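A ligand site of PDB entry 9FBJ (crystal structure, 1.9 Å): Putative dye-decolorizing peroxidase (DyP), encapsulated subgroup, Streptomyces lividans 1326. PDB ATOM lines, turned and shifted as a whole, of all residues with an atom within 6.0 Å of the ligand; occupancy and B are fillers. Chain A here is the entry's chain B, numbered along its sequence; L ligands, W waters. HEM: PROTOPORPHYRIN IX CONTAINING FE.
NE2 of His 225 is bound to FE of the ligand, 2.1 Å away. The backbone NH (N) of Gly 153 sits at hydrogen-bond distance from an oxygen (O1A) of the ligand. NH2 of Arg 243 lies within salt-bridge range of O1A of the ligand, 3.0 Å away. The backbone NH (N) of Glu 155 is in hydrogen-bond range of an oxygen (O2A) of the ligand (3.1 Å). N of Thr 154 lies within hydrogen-bond range of O1A of the ligand (3.3 Å).
O of His 225 is in hydrogen-bond range of OG1 of Thr 229, at 2.9 Å. The side-chain carboxylate (OD1) of Asp 152 lies within salt-bridge range of the guanidinium group (NH1) of Arg 243 (3.8 Å). OD2 of Asp 212 lies within hydrogen-bond range of OG1 of Thr 154 (2.8 Å). OD2 of Asp 146 sits close to OD2 of Asp 152, at 2.6 Å. OD1 of Asp 152 lies within hydrogen-bond range of ND2 of Asn 245. The side-chain hydroxyl of Thr 258 is in hydrogen-bond range of a ring nitrogen (NE2) of His 188, at 2.7 Å. OH of Tyr 186 is in hydrogen-bond range of OE1 of Gln 184 (2.5 Å). The backbone carbonyl oxygen (O) of Ile 205 lies within hydrogen-bond range of the backbone NH (N) of Val 226, at 3.0 Å.
Residues that only touch the ligand: Asp 146 (3.6 Å), Leu 148 (3.9 Å), Phe 150 (3.8 Å), Val 151 (3.3 Å), Asp 152 (3.4 Å), Gln 184 (3.5 Å), Tyr 186 (3.6 Å), His 188 (3.8 Å), Arg 207 (3.7 Å), Val 226 (3.6 Å), Thr 229 (3.3 Å), Ser 230 (3.9 Å), Asn 245 (3.8 Å), Thr 258 (3.4 Å), Phe 260 (3.4 Å), Met 273 (3.8 Å), Leu 274 (3.9 Å), Met 277 (3.7 Å), Ile 289 (3.6 Å) and Ser 293 (3.8 Å). Hydrophobic or aromatic side chains that line the ligand: Leu 148, Phe 150, Tyr 186, His 188, His 225, Val 226, Phe 260, Met 273, Leu 274, Met 277 and Ile 289.
Water W1 lies within hydrogen-bond range of O1D of the ligand and NH2 of Arg 207. Water W2 lies within hydrogen-bond range of an oxygen (O2D) of the ligand (3.0 Å) and the backbone carbonyl oxygen (O) of Thr 229 (3.1 Å).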
ATOM      1  N   ASP A 146      -8.750  21.248   4.624  1.00  0.00           N
ATOM      2  CA  ASP A 146      -9.708  22.236   4.106  1.00  0.00           C
ATOM      3  C   ASP A 146      -8.931  23.334   3.364  1.00  0.00           C
ATOM      4  O   ASP A 146      -7.717  23.175   3.126  1.00  0.00           O
ATOM      5  CB  ASP A 146     -10.579  22.743   5.245  1.00  0.00           C
ATOM      6  CG  ASP A 146      -9.845  23.397   6.417  1.00  0.00           C
ATOM      7  OD1 ASP A 146      -8.751  23.901   6.184  1.00  0.00           O
ATOM      8  OD2 ASP A 146     -10.406  23.429   7.562  1.00  0.00           O
ATOM      9  N   LEU A 148      -8.060  26.222   4.310  1.00  0.00           N
ATOM     10  CA  LEU A 148      -7.131  26.967   5.153  1.00  0.00           C
ATOM     11  C   LEU A 148      -5.861  26.156   5.378  1.00  0.00           C
ATOM     12  O   LEU A 148      -4.910  26.669   6.025  1.00  0.00           O
ATOM     13  CB  LEU A 148      -7.849  27.380   6.447  1.00  0.00           C
ATOM     14  CG  LEU A 148      -9.122  28.248   6.304  1.00  0.00           C
ATOM     15  CD1 LEU A 148      -9.607  28.649   7.670  1.00  0.00           C
ATOM     16  CD2 LEU A 148      -9.019  29.523   5.485  1.00  0.00           C
ATOM     17  N   PHE A 150      -5.710  23.280   7.071  1.00  0.00           N
ATOM     18  CA  PHE A 150      -5.811  22.475   8.292  1.00  0.00           C
ATOM     19  C   PHE A 150      -6.707  21.234   8.124  1.00  0.00           C
ATOM     20  O   PHE A 150      -7.694  21.244   7.419  1.00  0.00           O
ATOM     21  CB  PHE A 150      -6.385  23.263   9.470  1.00  0.00           C
ATOM     22  CG  PHE A 150      -5.403  24.236  10.127  1.00  0.00           C
ATOM     23  CD1 PHE A 150      -4.872  25.306   9.418  1.00  0.00           C
ATOM     24  CD2 PHE A 150      -5.043  24.104  11.467  1.00  0.00           C
ATOM     25  CE1 PHE A 150      -3.992  26.181  10.022  1.00  0.00           C
ATOM     26  CE2 PHE A 150      -4.108  24.950  12.034  1.00  0.00           C
ATOM     27  CZ  PHE A 150      -3.600  26.006  11.318  1.00  0.00           C
ATOM     28  N   VAL A 151      -6.377  20.187   8.908  1.00  0.00           N
ATOM     29  CA  VAL A 151      -7.115  18.928   8.970  1.00  0.00           C
ATOM     30  C   VAL A 151      -8.459  19.237   9.595  1.00  0.00           C
ATOM     31  O   VAL A 151      -8.533  19.919  10.595  1.00  0.00           O
ATOM     32  CB  VAL A 151      -6.370  17.796   9.687  1.00  0.00           C
ATOM     33  CG1 VAL A 151      -7.222  16.530   9.766  1.00  0.00           C
ATOM     34  CG2 VAL A 151      -5.019  17.516   9.065  1.00  0.00           C
ATOM     35  N   ASP A 152      -9.522  18.823   8.920  1.00  0.00           N
ATOM     36  CA  ASP A 152     -10.861  19.272   9.250  1.00  0.00           C
ATOM     37  C   ASP A 152     -11.769  18.051   9.407  1.00  0.00           C
ATOM     38  O   ASP A 152     -12.203  17.452   8.397  1.00  0.00           O
ATOM     39  CB  ASP A 152     -11.349  20.204   8.147  1.00  0.00           C
ATOM     40  CG  ASP A 152     -12.580  21.053   8.422  1.00  0.00           C
ATOM     41  OD1 ASP A 152     -13.455  20.565   9.076  1.00  0.00           O
ATOM     42  OD2 ASP A 152     -12.691  22.165   7.842  1.00  0.00           O
ATOM     43  N   GLY A 153     -12.160  17.765  10.660  1.00  0.00           N
ATOM     44  CA  GLY A 153     -13.036  16.641  10.954  1.00  0.00           C
ATOM     45  C   GLY A 153     -12.663  15.870  12.226  1.00  0.00           C
ATOM     46  O   GLY A 153     -13.462  15.075  12.760  1.00  0.00           O
ATOM     47  N   THR A 154     -11.441  16.135  12.683  1.00  0.00           N
ATOM     48  CA  THR A 154     -10.740  15.395  13.728  1.00  0.00           C
ATOM     49  C   THR A 154     -11.641  15.103  14.909  1.00  0.00           C
ATOM     50  O   THR A 154     -11.750  13.963  15.348  1.00  0.00           O
ATOM     51  CB  THR A 154      -9.521  16.179  14.213  1.00  0.00           C
ATOM     52  OG1 THR A 154      -8.868  16.586  13.015  1.00  0.00           O
ATOM     53  CG2 THR A 154      -8.718  15.358  15.207  1.00  0.00           C
ATOM     54  N   GLU A 155     -12.378  16.108  15.386  1.00  0.00           N
ATOM     55  CA  GLU A 155     -13.036  15.975  16.683  1.00  0.00           C
ATOM     56  C   GLU A 155     -14.485  15.543  16.506  1.00  0.00           C
ATOM     57  O   GLU A 155     -15.243  15.534  17.464  1.00  0.00           O
ATOM     58  CB  GLU A 155     -12.870  17.157  17.643  1.00  0.00           C
ATOM     59  CG  GLU A 155     -11.496  17.237  18.296  1.00  0.00           C
ATOM     60  CD  GLU A 155     -11.145  16.032  19.158  1.00  0.00           C
ATOM     61  OE1 GLU A 155     -11.869  15.882  20.149  1.00  0.00           O
ATOM     62  OE2 GLU A 155     -10.178  15.279  18.843  1.00  0.00           O
ATOM     63  N   ASN A 156     -14.851  15.086  15.294  1.00  0.00           N
ATOM     64  CA  ASN A 156     -16.224  14.646  15.112  1.00  0.00           C
ATOM     65  C   ASN A 156     -16.442  13.421  15.971  1.00  0.00           C
ATOM     66  O   ASN A 156     -15.531  12.570  16.073  1.00  0.00           O
ATOM     67  CB  ASN A 156     -16.579  14.245  13.688  1.00  0.00           C
ATOM     68  CG  ASN A 156     -16.967  15.383  12.779  1.00  0.00           C
ATOM     69  OD1 ASN A 156     -17.658  16.309  13.189  1.00  0.00           O
ATOM     70  ND2 ASN A 156     -16.606  15.257  11.530  1.00  0.00           N
ATOM     71  N   GLN A 184     -24.005  26.984   6.048  1.00  0.00           N
ATOM     72  CA  GLN A 184     -23.444  28.316   5.791  1.00  0.00           C
ATOM     73  C   GLN A 184     -22.333  28.186   4.762  1.00  0.00           C
ATOM     74  O   GLN A 184     -21.336  27.461   4.967  1.00  0.00           O
ATOM     75  CB  GLN A 184     -22.787  29.021   6.994  1.00  0.00           C
ATOM     76  CG  GLN A 184     -23.758  29.325   8.133  1.00  0.00           C
ATOM     77  CD  GLN A 184     -23.109  29.902   9.343  1.00  0.00           C
ATOM     78  OE1 GLN A 184     -22.180  29.327   9.900  1.00  0.00           O
ATOM     79  NE2 GLN A 184     -23.493  31.114   9.729  1.00  0.00           N
ATOM     80  N   TYR A 186     -19.180  29.740   3.249  1.00  0.00           N
ATOM     81  CA  TYR A 186     -18.223  30.756   3.623  1.00  0.00           C
ATOM     82  C   TYR A 186     -17.287  31.069   2.453  1.00  0.00           C
ATOM     83  O   TYR A 186     -16.731  30.116   1.879  1.00  0.00           O
ATOM     84  CB  TYR A 186     -17.444  30.340   4.862  1.00  0.00           C
ATOM     85  CG  TYR A 186     -18.134  30.470   6.207  1.00  0.00           C
ATOM     86  CD1 TYR A 186     -18.965  29.457   6.674  1.00  0.00           C
ATOM     87  CD2 TYR A 186     -18.106  31.663   6.916  1.00  0.00           C
ATOM     88  CE1 TYR A 186     -19.615  29.551   7.888  1.00  0.00           C
ATOM     89  CE2 TYR A 186     -18.733  31.782   8.149  1.00  0.00           C
ATOM     90  CZ  TYR A 186     -19.522  30.733   8.635  1.00  0.00           C
ATOM     91  OH  TYR A 186     -20.144  30.810   9.849  1.00  0.00           O
ATOM     92  N   HIS A 188     -13.476  32.838   1.870  1.00  0.00           N
ATOM     93  CA  HIS A 188     -12.247  33.169   2.541  1.00  0.00           C
ATOM     94  C   HIS A 188     -11.473  34.245   1.770  1.00  0.00           C
ATOM     95  O   HIS A 188     -11.503  34.364   0.533  1.00  0.00           O
ATOM     96  CB  HIS A 188     -11.411  31.884   2.664  1.00  0.00           C
ATOM     97  CG  HIS A 188     -12.055  30.791   3.414  1.00  0.00           C
ATOM     98  ND1 HIS A 188     -12.305  31.005   4.737  1.00  0.00           N
ATOM     99  CD2 HIS A 188     -12.479  29.559   3.141  1.00  0.00           C
ATOM    100  CE1 HIS A 188     -12.909  29.933   5.232  1.00  0.00           C
ATOM    101  NE2 HIS A 188     -13.034  29.041   4.309  1.00  0.00           N
ATOM    102  N   ILE A 205      -6.896  28.780  14.822  1.00  0.00           N
ATOM    103  CA  ILE A 205      -7.670  27.525  14.857  1.00  0.00           C
ATOM    104  C   ILE A 205      -7.643  26.933  16.279  1.00  0.00           C
ATOM    105  O   ILE A 205      -8.663  26.459  16.697  1.00  0.00           O
ATOM    106  CB  ILE A 205      -7.056  26.570  13.816  1.00  0.00           C
ATOM    107  CG1 ILE A 205      -7.158  27.174  12.385  1.00  0.00           C
ATOM    108  CG2 ILE A 205      -7.634  25.134  13.906  1.00  0.00           C
ATOM    109  CD1 ILE A 205      -8.559  27.549  11.969  1.00  0.00           C
ATOM    110  N   ARG A 207      -5.120  24.390  16.904  1.00  0.00           N
ATOM    111  CA  ARG A 207      -4.416  23.119  16.703  1.00  0.00           C
ATOM    112  C   ARG A 207      -3.148  23.328  15.894  1.00  0.00           C
ATOM    113  O   ARG A 207      -3.053  24.312  15.170  1.00  0.00           O
ATOM    114  CB  ARG A 207      -5.402  22.129  16.064  1.00  0.00           C
ATOM    115  CG  ARG A 207      -6.768  21.928  16.718  1.00  0.00           C
ATOM    116  CD  ARG A 207      -7.577  20.836  16.027  1.00  0.00           C
ATOM    117  NE  ARG A 207      -7.097  19.444  16.142  1.00  0.00           N
ATOM    118  CZ  ARG A 207      -7.422  18.663  17.190  1.00  0.00           C
ATOM    119  NH1 ARG A 207      -6.755  17.569  17.459  1.00  0.00           N
ATOM    120  NH2 ARG A 207      -8.403  19.008  17.982  1.00  0.00           N
ATOM    121  N   ASP A 212      -1.710  18.255  13.630  1.00  0.00           N
ATOM    122  CA  ASP A 212      -3.089  18.303  14.070  1.00  0.00           C
ATOM    123  C   ASP A 212      -3.242  17.945  15.543  1.00  0.00           C
ATOM    124  O   ASP A 212      -4.297  17.483  15.966  1.00  0.00           O
ATOM    125  CB  ASP A 212      -3.964  17.399  13.228  1.00  0.00           C
ATOM    126  CG  ASP A 212      -5.468  17.506  13.321  1.00  0.00           C
ATOM    127  OD1 ASP A 212      -5.985  18.606  13.616  1.00  0.00           O
ATOM    128  OD2 ASP A 212      -6.116  16.480  13.025  1.00  0.00           O
ATOM    129  N   GLU A 214      -3.906  19.102  19.344  1.00  0.00           N
ATOM    130  CA  GLU A 214      -4.563  20.265  19.931  1.00  0.00           C
ATOM    131  C   GLU A 214      -3.548  21.034  20.758  1.00  0.00           C
ATOM    132  O   GLU A 214      -2.618  20.437  21.308  1.00  0.00           O
ATOM    133  CB  GLU A 214      -5.763  19.808  20.741  1.00  0.00           C
ATOM    134  CG  GLU A 214      -6.658  20.942  21.265  1.00  0.00           C
ATOM    135  CD  GLU A 214      -7.767  20.471  22.168  1.00  0.00           C
ATOM    136  OE1 GLU A 214      -7.895  19.213  22.294  1.00  0.00           O
ATOM    137  OE2 GLU A 214      -8.468  21.343  22.776  1.00  0.00           O
ATOM    138  N   HIS A 225     -10.899  29.325  17.328  1.00  0.00           N
ATOM    139  CA  HIS A 225     -12.042  28.536  16.883  1.00  0.00           C
ATOM    140  C   HIS A 225     -12.359  27.333  17.791  1.00  0.00           C
ATOM    141  O   HIS A 225     -13.512  27.111  18.139  1.00  0.00           O
ATOM    142  CB  HIS A 225     -11.750  28.088  15.456  1.00  0.00           C
ATOM    143  CG  HIS A 225     -12.899  27.467  14.798  1.00  0.00           C
ATOM    144  ND1 HIS A 225     -14.139  28.013  14.666  1.00  0.00           N
ATOM    145  CD2 HIS A 225     -12.923  26.238  14.243  1.00  0.00           C
ATOM    146  CE1 HIS A 225     -14.905  27.122  14.039  1.00  0.00           C
ATOM    147  NE2 HIS A 225     -14.161  26.020  13.797  1.00  0.00           N
ATOM    148  N   VAL A 226     -11.371  26.467  18.073  1.00  0.00           N
ATOM    149  CA  VAL A 226     -11.626  25.313  18.938  1.00  0.00           C
ATOM    150  C   VAL A 226     -12.115  25.730  20.338  1.00  0.00           C
ATOM    151  O   VAL A 226     -13.015  25.064  20.855  1.00  0.00           O
ATOM    152  CB  VAL A 226     -10.439  24.346  19.031  1.00  0.00           C
ATOM    153  CG1 VAL A 226     -10.574  23.316  20.152  1.00  0.00           C
ATOM    154  CG2 VAL A 226     -10.218  23.660  17.711  1.00  0.00           C
ATOM    155  N   THR A 229     -15.868  26.951  20.107  1.00  0.00           N
ATOM    156  CA  THR A 229     -16.910  26.023  19.670  1.00  0.00           C
ATOM    157  C   THR A 229     -16.961  24.832  20.640  1.00  0.00           C
ATOM    158  O   THR A 229     -17.750  23.919  20.398  1.00  0.00           O
ATOM    159  CB  THR A 229     -16.772  25.600  18.195  1.00  0.00           C
ATOM    160  OG1 THR A 229     -15.499  25.056  17.872  1.00  0.00           O
ATOM    161  CG2 THR A 229     -17.019  26.767  17.250  1.00  0.00           C
ATOM    162  N   SER A 230     -16.149  24.880  21.727  1.00  0.00           N
ATOM    163  CA  SER A 230     -16.153  23.919  22.822  1.00  0.00           C
ATOM    164  C   SER A 230     -17.151  24.353  23.882  1.00  0.00           C
ATOM    165  O   SER A 230     -16.932  25.362  24.571  1.00  0.00           O
ATOM    166  CB  SER A 230     -14.766  23.743  23.449  1.00  0.00           C
ATOM    167  OG  SER A 230     -13.872  23.237  22.471  1.00  0.00           O
ATOM    168  N   ILE A 241     -21.496  18.323  17.831  1.00  0.00           N
ATOM    169  CA  ILE A 241     -22.202  18.206  16.563  1.00  0.00           C
ATOM    170  C   ILE A 241     -21.366  17.351  15.603  1.00  0.00           C
ATOM    171  O   ILE A 241     -20.216  17.134  15.881  1.00  0.00           O
ATOM    172  CB  ILE A 241     -22.520  19.551  15.933  1.00  0.00           C
ATOM    173  CG1 ILE A 241     -21.238  20.297  15.473  1.00  0.00           C
ATOM    174  CG2 ILE A 241     -23.331  20.424  16.889  1.00  0.00           C
ATOM    175  CD1 ILE A 241     -21.518  21.631  14.779  1.00  0.00           C
ATOM    176  N   ARG A 243     -19.979  17.286  11.734  1.00  0.00           N
ATOM    177  CA  ARG A 243     -19.680  18.238  10.655  1.00  0.00           C
ATOM    178  C   ARG A 243     -19.227  17.503   9.404  1.00  0.00           C
ATOM    179  O   ARG A 243     -18.485  16.520   9.530  1.00  0.00           O
ATOM    180  CB  ARG A 243     -18.545  19.174  11.133  1.00  0.00           C
ATOM    181  CG  ARG A 243     -19.021  20.233  12.115  1.00  0.00           C
ATOM    182  CD  ARG A 243     -17.920  20.935  12.967  1.00  0.00           C
ATOM    183  NE  ARG A 243     -17.047  19.979  13.673  1.00  0.00           N
ATOM    184  CZ  ARG A 243     -15.793  19.749  13.370  1.00  0.00           C
ATOM    185  NH1 ARG A 243     -15.183  20.439  12.416  1.00  0.00           N
ATOM    186  NH2 ARG A 243     -15.173  18.802  14.014  1.00  0.00           N
ATOM    187  N   ASN A 245     -17.674  19.508   6.451  1.00  0.00           N
ATOM    188  CA  ASN A 245     -17.321  20.727   5.740  1.00  0.00           C
ATOM    189  C   ASN A 245     -16.572  20.421   4.444  1.00  0.00           C
ATOM    190  O   ASN A 245     -15.730  19.517   4.364  1.00  0.00           O
ATOM    191  CB  ASN A 245     -16.302  21.538   6.557  1.00  0.00           C
ATOM    192  CG  ASN A 245     -16.880  22.046   7.850  1.00  0.00           C
ATOM    193  OD1 ASN A 245     -18.100  21.999   8.051  1.00  0.00           O
ATOM    194  ND2 ASN A 245     -16.018  22.491   8.752  1.00  0.00           N
ATOM    195  N   THR A 258     -15.303  27.443   2.114  1.00  0.00           N
ATOM    196  CA  THR A 258     -15.702  26.298   2.928  1.00  0.00           C
ATOM    197  C   THR A 258     -17.229  26.271   3.002  1.00  0.00           C
ATOM    198  O   THR A 258     -17.869  27.211   3.461  1.00  0.00           O
ATOM    199  CB  THR A 258     -15.122  26.363   4.353  1.00  0.00           C
ATOM    200  OG1 THR A 258     -13.706  26.422   4.367  1.00  0.00           O
ATOM    201  CG2 THR A 258     -15.495  25.106   5.139  1.00  0.00           C
ATOM    202  N   PHE A 260     -19.896  24.947   5.107  1.00  0.00           N
ATOM    203  CA  PHE A 260     -20.195  24.396   6.420  1.00  0.00           C
ATOM    204  C   PHE A 260     -21.536  23.653   6.417  1.00  0.00           C
ATOM    205  O   PHE A 260     -22.531  24.229   6.021  1.00  0.00           O
ATOM    206  CB  PHE A 260     -20.335  25.530   7.449  1.00  0.00           C
ATOM    207  CG  PHE A 260     -20.778  25.042   8.815  1.00  0.00           C
ATOM    208  CD1 PHE A 260     -19.905  24.388   9.682  1.00  0.00           C
ATOM    209  CD2 PHE A 260     -22.066  25.313   9.244  1.00  0.00           C
ATOM    210  CE1 PHE A 260     -20.391  23.907  10.909  1.00  0.00           C
ATOM    211  CE2 PHE A 260     -22.526  24.816  10.449  1.00  0.00           C
ATOM    212  CZ  PHE A 260     -21.669  24.201  11.316  1.00  0.00           C
ATOM    213  N   THR A 270     -26.102  23.870  17.924  1.00  0.00           N
ATOM    214  CA  THR A 270     -25.467  24.592  16.813  1.00  0.00           C
ATOM    215  C   THR A 270     -25.580  26.115  16.960  1.00  0.00           C
ATOM    216  O   THR A 270     -24.634  26.863  16.713  1.00  0.00           O
ATOM    217  CB  THR A 270     -26.088  24.175  15.489  1.00  0.00           C
ATOM    218  OG1 THR A 270     -25.991  22.757  15.377  1.00  0.00           O
ATOM    219  CG2 THR A 270     -25.356  24.848  14.336  1.00  0.00           C
ATOM    220  N   MET A 273     -23.214  27.582  19.588  1.00  0.00           N
ATOM    221  CA  MET A 273     -21.844  27.637  19.087  1.00  0.00           C
ATOM    222  C   MET A 273     -21.704  28.885  18.207  1.00  0.00           C
ATOM    223  O   MET A 273     -20.662  29.565  18.313  1.00  0.00           O
ATOM    224  CB  MET A 273     -21.504  26.383  18.272  1.00  0.00           C
ATOM    225  CG  MET A 273     -21.332  25.141  19.064  1.00  0.00           C
ATOM    226  SD  MET A 273     -20.959  23.691  18.028  1.00  0.00           S
ATOM    227  CE  MET A 273     -20.553  22.661  19.447  1.00  0.00           C
ATOM    228  N   LEU A 274     -22.705  29.101  17.321  1.00  0.00           N
ATOM    229  CA  LEU A 274     -22.844  30.235  16.429  1.00  0.00           C
ATOM    230  C   LEU A 274     -22.881  31.522  17.259  1.00  0.00           C
ATOM    231  O   LEU A 274     -22.290  32.524  16.831  1.00  0.00           O
ATOM    232  CB  LEU A 274     -24.075  30.175  15.523  1.00  0.00           C
ATOM    233  CG  LEU A 274     -23.911  29.302  14.281  1.00  0.00           C
ATOM    234  CD1 LEU A 274     -25.256  29.042  13.589  1.00  0.00           C
ATOM    235  CD2 LEU A 274     -22.855  29.871  13.308  1.00  0.00           C
ATOM    236  N   MET A 277     -19.323  32.260  18.470  1.00  0.00           N
ATOM    237  CA  MET A 277     -18.544  32.675  17.295  1.00  0.00           C
ATOM    238  C   MET A 277     -18.755  34.158  16.938  1.00  0.00           C
ATOM    239  O   MET A 277     -17.782  34.897  16.782  1.00  0.00           O
ATOM    240  CB  MET A 277     -18.861  31.775  16.085  1.00  0.00           C
ATOM    241  CG  MET A 277     -18.146  30.391  16.234  1.00  0.00           C
ATOM    242  SD  MET A 277     -18.527  29.418  14.762  1.00  0.00           S
ATOM    243  CE  MET A 277     -17.575  30.220  13.443  1.00  0.00           C
ATOM    244  N   PHE A 278     -20.011  34.575  16.782  1.00  0.00           N
ATOM    245  CA  PHE A 278     -20.360  35.858  16.181  1.00  0.00           C
ATOM    246  C   PHE A 278     -20.520  36.965  17.214  1.00  0.00           C
ATOM    247  O   PHE A 278     -20.223  38.115  16.891  1.00  0.00           O
ATOM    248  CB  PHE A 278     -21.610  35.679  15.319  1.00  0.00           C
ATOM    249  CG  PHE A 278     -21.341  35.032  13.966  1.00  0.00           C
ATOM    250  CD1 PHE A 278     -21.331  33.645  13.825  1.00  0.00           C
ATOM    251  CD2 PHE A 278     -21.127  35.811  12.838  1.00  0.00           C
ATOM    252  CE1 PHE A 278     -21.042  33.063  12.598  1.00  0.00           C
ATOM    253  CE2 PHE A 278     -20.853  35.220  11.599  1.00  0.00           C
ATOM    254  CZ  PHE A 278     -20.858  33.856  11.484  1.00  0.00           C
ATOM    255  N   ILE A 289     -11.503  33.019  13.351  1.00  0.00           N
ATOM    256  CA  ILE A 289     -11.672  32.464  11.996  1.00  0.00           C
ATOM    257  C   ILE A 289     -12.544  33.394  11.155  1.00  0.00           C
ATOM    258  O   ILE A 289     -12.503  33.440   9.917  1.00  0.00           O
ATOM    259  CB  ILE A 289     -12.156  30.995  12.077  1.00  0.00           C
ATOM    260  CG1 ILE A 289     -11.645  30.111  10.928  1.00  0.00           C
ATOM    261  CG2 ILE A 289     -13.665  30.981  12.150  1.00  0.00           C
ATOM    262  CD1 ILE A 289     -12.159  28.681  10.949  1.00  0.00           C
ATOM    263  N   SER A 293     -12.975  34.884   7.108  1.00  0.00           N
ATOM    264  CA  SER A 293     -14.106  34.092   6.657  1.00  0.00           C
ATOM    265  C   SER A 293     -15.385  34.914   6.619  1.00  0.00           C
ATOM    266  O   SER A 293     -15.810  35.412   7.659  1.00  0.00           O
ATOM    267  CB  SER A 293     -14.277  32.863   7.514  1.00  0.00           C
ATOM    268  OG  SER A 293     -13.130  32.006   7.446  1.00  0.00           O
HETATM  269  CHA HEM L   1     -13.308  22.283  14.601  1.00  0.00           C
HETATM  270  CHB HEM L   1     -12.530  24.475  10.336  1.00  0.00           C
HETATM  271  CHC HEM L   1     -16.795  26.715  10.758  1.00  0.00           C
HETATM  272  CHD HEM L   1     -17.779  24.133  14.691  1.00  0.00           C
HETATM  273  C1A HEM L   1     -12.691  22.745  13.435  1.00  0.00           C
HETATM  274  C2A HEM L   1     -11.385  22.400  13.010  1.00  0.00           C
HETATM  275  C3A HEM L   1     -11.158  22.994  11.877  1.00  0.00           C
HETATM  276  C4A HEM L   1     -12.331  23.722  11.525  1.00  0.00           C
HETATM  277  CMA HEM L   1      -9.833  22.956  11.096  1.00  0.00           C
HETATM  278  CAA HEM L   1     -10.365  21.602  13.734  1.00  0.00           C
HETATM  279  CBA HEM L   1     -10.310  20.128  13.495  1.00  0.00           C
HETATM  280  CGA HEM L   1     -11.630  19.531  13.798  1.00  0.00           C
HETATM  281  O1A HEM L   1     -12.443  19.258  12.870  1.00  0.00           O
HETATM  282  O2A HEM L   1     -11.924  19.094  14.890  1.00  0.00           O
HETATM  283  C1B HEM L   1     -13.665  25.306  10.035  1.00  0.00           C
HETATM  284  C2B HEM L   1     -13.843  26.265   8.864  1.00  0.00           C
HETATM  285  C3B HEM L   1     -15.022  26.860   9.046  1.00  0.00           C
HETATM  286  C4B HEM L   1     -15.561  26.276  10.309  1.00  0.00           C
HETATM  287  CMB HEM L   1     -12.899  26.511   7.691  1.00  0.00           C
HETATM  288  CAB HEM L   1     -15.883  27.910   8.487  1.00  0.00           C
HETATM  289  CBB HEM L   1     -15.381  28.919   7.875  1.00  0.00           C
HETATM  290  C1C HEM L   1     -17.436  26.174  11.860  1.00  0.00           C
HETATM  291  C2C HEM L   1     -18.714  26.592  12.325  1.00  0.00           C
HETATM  292  C3C HEM L   1     -19.052  25.841  13.432  1.00  0.00           C
HETATM  293  C4C HEM L   1     -17.858  24.971  13.628  1.00  0.00           C
HETATM  294  CMC HEM L   1     -19.679  27.508  11.629  1.00  0.00           C
HETATM  295  CAC HEM L   1     -20.288  25.770  14.279  1.00  0.00           C
HETATM  296  CBC HEM L   1     -21.444  26.339  14.212  1.00  0.00           C
HETATM  297  C1D HEM L   1     -16.642  23.406  14.970  1.00  0.00           C
HETATM  298  C2D HEM L   1     -16.586  22.426  16.130  1.00  0.00           C
HETATM  299  C3D HEM L   1     -15.373  21.965  16.088  1.00  0.00           C
HETATM  300  C4D HEM L   1     -14.671  22.618  14.932  1.00  0.00           C
HETATM  301  CMD HEM L   1     -17.569  22.106  17.223  1.00  0.00           C
HETATM  302  CAD HEM L   1     -14.759  21.072  17.105  1.00  0.00           C
HETATM  303  CBD HEM L   1     -14.141  21.782  18.340  1.00  0.00           C
HETATM  304  CGD HEM L   1     -13.512  20.747  19.319  1.00  0.00           C
HETATM  305  O1D HEM L   1     -12.300  20.289  19.323  1.00  0.00           O
HETATM  306  O2D HEM L   1     -14.282  20.209  20.110  1.00  0.00           O
HETATM  307  NA  HEM L   1     -13.301  23.466  12.437  1.00  0.00           N
HETATM  308  NB  HEM L   1     -14.721  25.366  10.829  1.00  0.00           N
HETATM  309  NC  HEM L   1     -16.858  25.304  12.742  1.00  0.00           N
HETATM  310  ND  HEM L   1     -15.497  23.524  14.278  1.00  0.00           N
HETATM  311 FE   HEM L   1     -15.078  24.465  12.665  1.00  0.00          FE
HETATM  312  O   HOH W   1     -10.885  20.567  17.202  1.00  0.00           O
HETATM  313  O   HOH W   2     -17.206  20.849  20.365  1.00  0.00           O
